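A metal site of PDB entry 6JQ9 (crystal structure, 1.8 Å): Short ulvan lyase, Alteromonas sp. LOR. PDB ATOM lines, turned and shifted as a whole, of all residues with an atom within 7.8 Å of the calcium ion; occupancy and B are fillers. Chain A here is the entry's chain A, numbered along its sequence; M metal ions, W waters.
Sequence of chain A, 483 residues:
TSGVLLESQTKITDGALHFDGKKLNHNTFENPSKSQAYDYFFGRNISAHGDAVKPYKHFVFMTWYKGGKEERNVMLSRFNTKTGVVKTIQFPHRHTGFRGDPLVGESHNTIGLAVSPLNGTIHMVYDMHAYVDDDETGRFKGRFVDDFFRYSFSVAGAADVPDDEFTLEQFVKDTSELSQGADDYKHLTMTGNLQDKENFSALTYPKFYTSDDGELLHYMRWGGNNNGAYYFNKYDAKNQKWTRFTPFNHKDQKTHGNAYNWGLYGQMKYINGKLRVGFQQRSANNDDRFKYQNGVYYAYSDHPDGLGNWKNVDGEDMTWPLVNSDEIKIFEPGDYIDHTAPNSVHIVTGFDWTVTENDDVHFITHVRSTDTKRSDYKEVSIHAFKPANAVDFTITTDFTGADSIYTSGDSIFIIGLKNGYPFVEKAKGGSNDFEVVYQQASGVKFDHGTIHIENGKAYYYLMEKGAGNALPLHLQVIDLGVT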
ATOM      1  N   VAL A 145      23.370 -23.558  -6.120  1.00  0.00           N
ATOM      2  CA  VAL A 145      22.282 -24.503  -5.794  1.00  0.00           C
ATOM      3  C   VAL A 145      21.385 -23.838  -4.731  1.00  0.00           C
ATOM      4  O   VAL A 145      21.873 -23.373  -3.669  1.00  0.00           O
ATOM      5  CB  VAL A 145      22.827 -25.885  -5.406  1.00  0.00           C
ATOM      6  CG1 VAL A 145      21.750 -26.777  -4.813  1.00  0.00           C
ATOM      7  CG2 VAL A 145      23.489 -26.558  -6.593  1.00  0.00           C
ATOM      8  N   ASP A 146      20.098 -23.771  -5.040  1.00  0.00           N
ATOM      9  CA  ASP A 146      19.015 -23.241  -4.162  1.00  0.00           C
ATOM     10  C   ASP A 146      19.247 -21.739  -3.907  1.00  0.00           C
ATOM     11  O   ASP A 146      18.711 -21.238  -2.895  1.00  0.00           O
ATOM     12  CB  ASP A 146      18.929 -24.006  -2.823  1.00  0.00           C
ATOM     13  CG  ASP A 146      18.684 -25.509  -2.934  1.00  0.00           C
ATOM     14  OD1 ASP A 146      18.295 -25.959  -4.006  1.00  0.00           O
ATOM     15  OD2 ASP A 146      18.953 -26.231  -1.926  1.00  0.00           O
ATOM     16  N   ASP A 147      19.996 -21.032  -4.766  1.00  0.00           N
ATOM     17  CA  ASP A 147      20.431 -19.631  -4.481  1.00  0.00           C
ATOM     18  C   ASP A 147      20.789 -18.923  -5.794  1.00  0.00           C
ATOM     19  O   ASP A 147      21.665 -18.066  -5.763  1.00  0.00           O
ATOM     20  CB  ASP A 147      21.613 -19.607  -3.539  1.00  0.00           C
ATOM     21  CG  ASP A 147      21.914 -18.249  -2.925  1.00  0.00           C
ATOM     22  OD1 ASP A 147      20.965 -17.520  -2.547  1.00  0.00           O
ATOM     23  OD2 ASP A 147      23.072 -17.932  -2.850  1.00  0.00           O
ATOM     24  N   PHE A 149      18.635 -17.240  -7.800  1.00  0.00           N
ATOM     25  CA  PHE A 149      17.837 -16.005  -7.846  1.00  0.00           C
ATOM     26  C   PHE A 149      17.842 -15.543  -6.396  1.00  0.00           C
ATOM     27  O   PHE A 149      17.598 -16.423  -5.522  1.00  0.00           O
ATOM     28  CB  PHE A 149      16.416 -16.256  -8.395  1.00  0.00           C
ATOM     29  CG  PHE A 149      15.601 -15.009  -8.611  1.00  0.00           C
ATOM     30  CD1 PHE A 149      15.033 -14.311  -7.550  1.00  0.00           C
ATOM     31  CD2 PHE A 149      15.414 -14.503  -9.889  1.00  0.00           C
ATOM     32  CE1 PHE A 149      14.270 -13.174  -7.765  1.00  0.00           C
ATOM     33  CE2 PHE A 149      14.701 -13.329 -10.090  1.00  0.00           C
ATOM     34  CZ  PHE A 149      14.133 -12.667  -9.045  1.00  0.00           C
ATOM     35  N   ARG A 150      18.187 -14.263  -6.162  1.00  0.00           N
ATOM     36  CA  ARG A 150      18.455 -13.664  -4.816  1.00  0.00           C
ATOM     37  C   ARG A 150      17.562 -12.440  -4.531  1.00  0.00           C
ATOM     38  O   ARG A 150      17.851 -11.390  -4.986  1.00  0.00           O
ATOM     39  CB  ARG A 150      19.956 -13.351  -4.685  1.00  0.00           C
ATOM     40  CG  ARG A 150      20.869 -14.534  -4.963  1.00  0.00           C
ATOM     41  CD  ARG A 150      22.356 -14.281  -5.179  1.00  0.00           C
ATOM     42  NE  ARG A 150      23.213 -15.413  -4.878  1.00  0.00           N
ATOM     43  CZ  ARG A 150      24.527 -15.507  -5.081  1.00  0.00           C
ATOM     44  NH1 ARG A 150      25.201 -14.567  -5.706  1.00  0.00           N
ATOM     45  NH2 ARG A 150      25.167 -16.579  -4.674  1.00  0.00           N
ATOM     46  N   TYR A 151      16.520 -12.677  -3.757  1.00  0.00           N
ATOM     47  CA  TYR A 151      15.482 -11.674  -3.446  1.00  0.00           C
ATOM     48  C   TYR A 151      15.386 -11.508  -1.928  1.00  0.00           C
ATOM     49  O   TYR A 151      15.207 -12.521  -1.219  1.00  0.00           O
ATOM     50  CB  TYR A 151      14.152 -12.101  -4.069  1.00  0.00           C
ATOM     51  CG  TYR A 151      12.922 -11.310  -3.681  1.00  0.00           C
ATOM     52  CD1 TYR A 151      12.860  -9.932  -3.777  1.00  0.00           C
ATOM     53  CD2 TYR A 151      11.781 -11.990  -3.284  1.00  0.00           C
ATOM     54  CE1 TYR A 151      11.709  -9.222  -3.451  1.00  0.00           C
ATOM     55  CE2 TYR A 151      10.619 -11.299  -2.989  1.00  0.00           C
ATOM     56  CZ  TYR A 151      10.578  -9.924  -3.077  1.00  0.00           C
ATOM     57  OH  TYR A 151       9.429  -9.281  -2.728  1.00  0.00           O
ATOM     58  N   LYS A 173      13.052 -13.643   6.588  1.00  0.00           N
ATOM     59  CA  LYS A 173      14.065 -14.706   6.382  1.00  0.00           C
ATOM     60  C   LYS A 173      13.476 -15.805   5.473  1.00  0.00           C
ATOM     61  O   LYS A 173      12.243 -15.950   5.383  1.00  0.00           O
ATOM     62  CB  LYS A 173      14.566 -15.293   7.717  1.00  0.00           C
ATOM     63  CG  LYS A 173      15.670 -14.441   8.374  1.00  0.00           C
ATOM     64  CD  LYS A 173      16.424 -15.146   9.485  1.00  0.00           C
ATOM     65  CE  LYS A 173      16.619 -14.271  10.687  1.00  0.00           C
ATOM     66  NZ  LYS A 173      17.087 -15.055  11.854  1.00  0.00           N
ATOM     67  N   ASP A 174      14.361 -16.513   4.788  1.00  0.00           N
ATOM     68  CA  ASP A 174      14.042 -17.753   4.041  1.00  0.00           C
ATOM     69  C   ASP A 174      13.860 -18.887   5.058  1.00  0.00           C
ATOM     70  O   ASP A 174      14.874 -19.288   5.635  1.00  0.00           O
ATOM     71  CB  ASP A 174      15.136 -18.103   3.036  1.00  0.00           C
ATOM     72  CG  ASP A 174      14.792 -19.316   2.182  1.00  0.00           C
ATOM     73  OD1 ASP A 174      13.767 -19.974   2.483  1.00  0.00           O
ATOM     74  OD2 ASP A 174      15.557 -19.617   1.239  1.00  0.00           O
ATOM     75  N   THR A 175      12.616 -19.337   5.269  1.00  0.00           N
ATOM     76  CA  THR A 175      12.248 -20.479   6.160  1.00  0.00           C
ATOM     77  C   THR A 175      11.673 -21.629   5.314  1.00  0.00           C
ATOM     78  O   THR A 175      11.066 -22.529   5.900  1.00  0.00           O
ATOM     79  CB  THR A 175      11.316 -19.993   7.275  1.00  0.00           C
ATOM     80  OG1 THR A 175      10.166 -19.390   6.667  1.00  0.00           O
ATOM     81  CG2 THR A 175      11.959 -18.995   8.212  1.00  0.00           C
ATOM     82  N   SER A 176      11.854 -21.591   3.998  1.00  0.00           N
ATOM     83  CA  SER A 176      11.562 -22.668   3.016  1.00  0.00           C
ATOM     84  C   SER A 176      12.352 -23.949   3.328  1.00  0.00           C
ATOM     85  O   SER A 176      13.308 -23.902   4.127  1.00  0.00           O
ATOM     86  CB  SER A 176      11.840 -22.201   1.584  1.00  0.00           C
ATOM     87  OG  SER A 176      13.210 -22.365   1.247  1.00  0.00           O
ATOM     88  N   LEU A 178      14.293 -25.148   1.398  1.00  0.00           N
ATOM     89  CA  LEU A 178      15.622 -24.937   0.752  1.00  0.00           C
ATOM     90  C   LEU A 178      16.447 -23.900   1.532  1.00  0.00           C
ATOM     91  O   LEU A 178      17.604 -23.668   1.103  1.00  0.00           O
ATOM     92  CB  LEU A 178      15.429 -24.513  -0.708  1.00  0.00           C
ATOM     93  CG  LEU A 178      14.698 -25.512  -1.619  1.00  0.00           C
ATOM     94  CD1 LEU A 178      14.724 -25.019  -3.058  1.00  0.00           C
ATOM     95  CD2 LEU A 178      15.320 -26.901  -1.524  1.00  0.00           C
ATOM     96  N   SER A 179      15.956 -23.390   2.667  1.00  0.00           N
ATOM     97  CA  SER A 179      16.675 -22.411   3.525  1.00  0.00           C
ATOM     98  C   SER A 179      18.128 -22.865   3.788  1.00  0.00           C
ATOM     99  O   SER A 179      18.348 -24.044   4.167  1.00  0.00           O
ATOM    100  CB  SER A 179      15.968 -22.174   4.843  1.00  0.00           C
ATOM    101  OG  SER A 179      16.718 -21.280   5.671  1.00  0.00           O
ATOM    102  N   GLN A 180      19.084 -21.949   3.643  1.00  0.00           N
ATOM    103  CA  GLN A 180      20.498 -22.222   4.015  1.00  0.00           C
ATOM    104  C   GLN A 180      20.726 -21.840   5.494  1.00  0.00           C
ATOM    105  O   GLN A 180      21.866 -21.880   5.911  1.00  0.00           O
ATOM    106  CB  GLN A 180      21.442 -21.473   3.065  1.00  0.00           C
ATOM    107  CG  GLN A 180      21.184 -21.833   1.609  1.00  0.00           C
ATOM    108  CD  GLN A 180      22.007 -20.991   0.676  1.00  0.00           C
ATOM    109  OE1 GLN A 180      21.871 -19.765   0.623  1.00  0.00           O
ATOM    110  NE2 GLN A 180      22.879 -21.661  -0.068  1.00  0.00           N
ATOM    111  N   GLY A 181      19.680 -21.456   6.236  1.00  0.00           N
ATOM    112  CA  GLY A 181      19.754 -21.404   7.714  1.00  0.00           C
ATOM    113  C   GLY A 181      19.434 -20.046   8.329  1.00  0.00           C
ATOM    114  O   GLY A 181      18.759 -19.251   7.685  1.00  0.00           O
ATOM    115  N   ASP A 183      20.648 -17.263   8.982  1.00  0.00           N
ATOM    116  CA  ASP A 183      21.129 -15.971   8.431  1.00  0.00           C
ATOM    117  C   ASP A 183      20.741 -15.837   6.957  1.00  0.00           C
ATOM    118  O   ASP A 183      21.273 -14.933   6.267  1.00  0.00           O
ATOM    119  CB  ASP A 183      22.644 -15.900   8.537  1.00  0.00           C
ATOM    120  CG  ASP A 183      23.410 -16.936   7.728  1.00  0.00           C
ATOM    121  OD1 ASP A 183      22.845 -18.036   7.369  1.00  0.00           O
ATOM    122  OD2 ASP A 183      24.572 -16.633   7.431  1.00  0.00           O
ATOM    123  N   ASP A 184      19.905 -16.746   6.447  1.00  0.00           N
ATOM    124  CA  ASP A 184      19.531 -16.737   5.003  1.00  0.00           C
ATOM    125  C   ASP A 184      18.333 -15.810   4.813  1.00  0.00           C
ATOM    126  O   ASP A 184      17.200 -16.133   5.320  1.00  0.00           O
ATOM    127  CB  ASP A 184      19.357 -18.169   4.502  1.00  0.00           C
ATOM    128  CG  ASP A 184      18.748 -18.297   3.117  1.00  0.00           C
ATOM    129  OD1 ASP A 184      18.596 -17.250   2.430  1.00  0.00           O
ATOM    130  OD2 ASP A 184      18.403 -19.439   2.726  1.00  0.00           O
ATOM    131  N   TYR A 185      18.560 -14.661   4.143  1.00  0.00           N
ATOM    132  CA  TYR A 185      17.536 -13.630   3.848  1.00  0.00           C
ATOM    133  C   TYR A 185      17.219 -13.639   2.349  1.00  0.00           C
ATOM    134  O   TYR A 185      16.442 -12.746   1.922  1.00  0.00           O
ATOM    135  CB  TYR A 185      18.017 -12.226   4.265  1.00  0.00           C
ATOM    136  CG  TYR A 185      17.845 -11.915   5.733  1.00  0.00           C
ATOM    137  CD1 TYR A 185      18.824 -12.226   6.662  1.00  0.00           C
ATOM    138  CD2 TYR A 185      16.663 -11.336   6.197  1.00  0.00           C
ATOM    139  CE1 TYR A 185      18.648 -11.954   8.023  1.00  0.00           C
ATOM    140  CE2 TYR A 185      16.486 -11.024   7.544  1.00  0.00           C
ATOM    141  CZ  TYR A 185      17.464 -11.362   8.460  1.00  0.00           C
ATOM    142  OH  TYR A 185      17.246 -11.034   9.795  1.00  0.00           O
ATOM    143  N   LYS A 186      17.746 -14.616   1.602  1.00  0.00           N
ATOM    144  CA  LYS A 186      17.641 -14.661   0.108  1.00  0.00           C
ATOM    145  C   LYS A 186      16.592 -15.692  -0.305  1.00  0.00           C
ATOM    146  O   LYS A 186      16.856 -16.875  -0.084  1.00  0.00           O
ATOM    147  CB  LYS A 186      18.942 -15.090  -0.559  1.00  0.00           C
ATOM    148  CG  LYS A 186      20.051 -14.073  -0.377  1.00  0.00           C
ATOM    149  CD  LYS A 186      21.322 -14.601  -0.856  1.00  0.00           C
ATOM    150  CE  LYS A 186      21.956 -15.525   0.160  1.00  0.00           C
ATOM    151  NZ  LYS A 186      23.184 -16.115  -0.401  1.00  0.00           N
ATOM    152  N   HIS A 187      15.504 -15.200  -0.912  1.00  0.00           N
ATOM    153  CA  HIS A 187      14.345 -15.956  -1.444  1.00  0.00           C
ATOM    154  C   HIS A 187      14.628 -16.336  -2.905  1.00  0.00           C
ATOM    155  O   HIS A 187      15.138 -15.474  -3.669  1.00  0.00           O
ATOM    156  CB  HIS A 187      13.074 -15.114  -1.261  1.00  0.00           C
ATOM    157  CG  HIS A 187      12.733 -14.910   0.177  1.00  0.00           C
ATOM    158  ND1 HIS A 187      11.941 -15.812   0.860  1.00  0.00           N
ATOM    159  CD2 HIS A 187      13.145 -13.994   1.077  1.00  0.00           C
ATOM    160  CE1 HIS A 187      11.859 -15.437   2.120  1.00  0.00           C
ATOM    161  NE2 HIS A 187      12.574 -14.312   2.284  1.00  0.00           N
ATOM    162  N   LEU A 188      14.265 -17.562  -3.279  1.00  0.00           N
ATOM    163  CA  LEU A 188      14.617 -18.107  -4.622  1.00  0.00           C
ATOM    164  C   LEU A 188      13.543 -17.707  -5.648  1.00  0.00           C
ATOM    165  O   LEU A 188      13.841 -17.730  -6.833  1.00  0.00           O
ATOM    166  CB  LEU A 188      14.775 -19.612  -4.446  1.00  0.00           C
ATOM    167  CG  LEU A 188      15.278 -20.387  -5.650  1.00  0.00           C
ATOM    168  CD1 LEU A 188      16.628 -19.830  -6.114  1.00  0.00           C
ATOM    169  CD2 LEU A 188      15.384 -21.846  -5.285  1.00  0.00           C
ATOM    170  N   LEU A 194       8.044 -22.147  -4.082  1.00  0.00           N
ATOM    171  CA  LEU A 194       9.241 -22.801  -4.693  1.00  0.00           C
ATOM    172  C   LEU A 194       8.852 -23.614  -5.933  1.00  0.00           C
ATOM    173  O   LEU A 194       9.764 -23.922  -6.743  1.00  0.00           O
ATOM    174  CB  LEU A 194       9.935 -23.715  -3.676  1.00  0.00           C
ATOM    175  CG  LEU A 194      10.602 -22.980  -2.530  1.00  0.00           C
ATOM    176  CD1 LEU A 194      10.931 -23.961  -1.414  1.00  0.00           C
ATOM    177  CD2 LEU A 194      11.848 -22.260  -3.013  1.00  0.00           C
HETATM  178 CA    CA M   1      17.635 -18.831   0.588  1.00  0.00          CA
HETATM  179  O   HOH W   1      17.214 -19.046  -1.797  1.00  0.00           O
HETATM  180  O   HOH W   2      20.219 -18.368  -0.317  1.00  0.00           O
HETATM  181  O   HOH W   3      18.257 -21.225  -0.027  1.00  0.00           O
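The side-chain carboxylate (OD2) of Asp 147 is in salt-bridge range of the side-chain amino group (NZ) of Lys 186, at 3.1 Å.
O of Asp 174 is in hydrogen-bond range of OG of Ser 179, 2.7 Å away.
The side-chain carboxylate of Asp 184 lies close to the backbone NH of Gln 180 (2.8 Å).
OD1 of Asp 174 is in hydrogen-bond range of OG of Ser 176, at 2.7 Å.
The nearest printed residue that does not touch the calcium ion is Gln 180 (4.3 Å).
The calcium ion is bound by the backbone carbonyl oxygen (O) of Lys 186 (2.2 Å).
The calcium ion is bound by OD2 of Asp 174 (2.3 Å).
OD2 of Asp 184 is bound to the calcium ion (2.4 Å).
The calcium ion is bound by water W1, 2.4 Å away.
Water W3 binds the calcium ion (2.5 Å).
OD1 of Asp 184 is bound to the calcium ion (2.6 Å).
Water W2 binds the calcium ion (2.8 Å).
Water W3 lies within hydrogen-bond range of the backbone carbonyl oxygen (O) of Leu 178 (2.8 Å) and the backbone carbonyl oxygen (O) of Asp 146 (2.9 Å).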
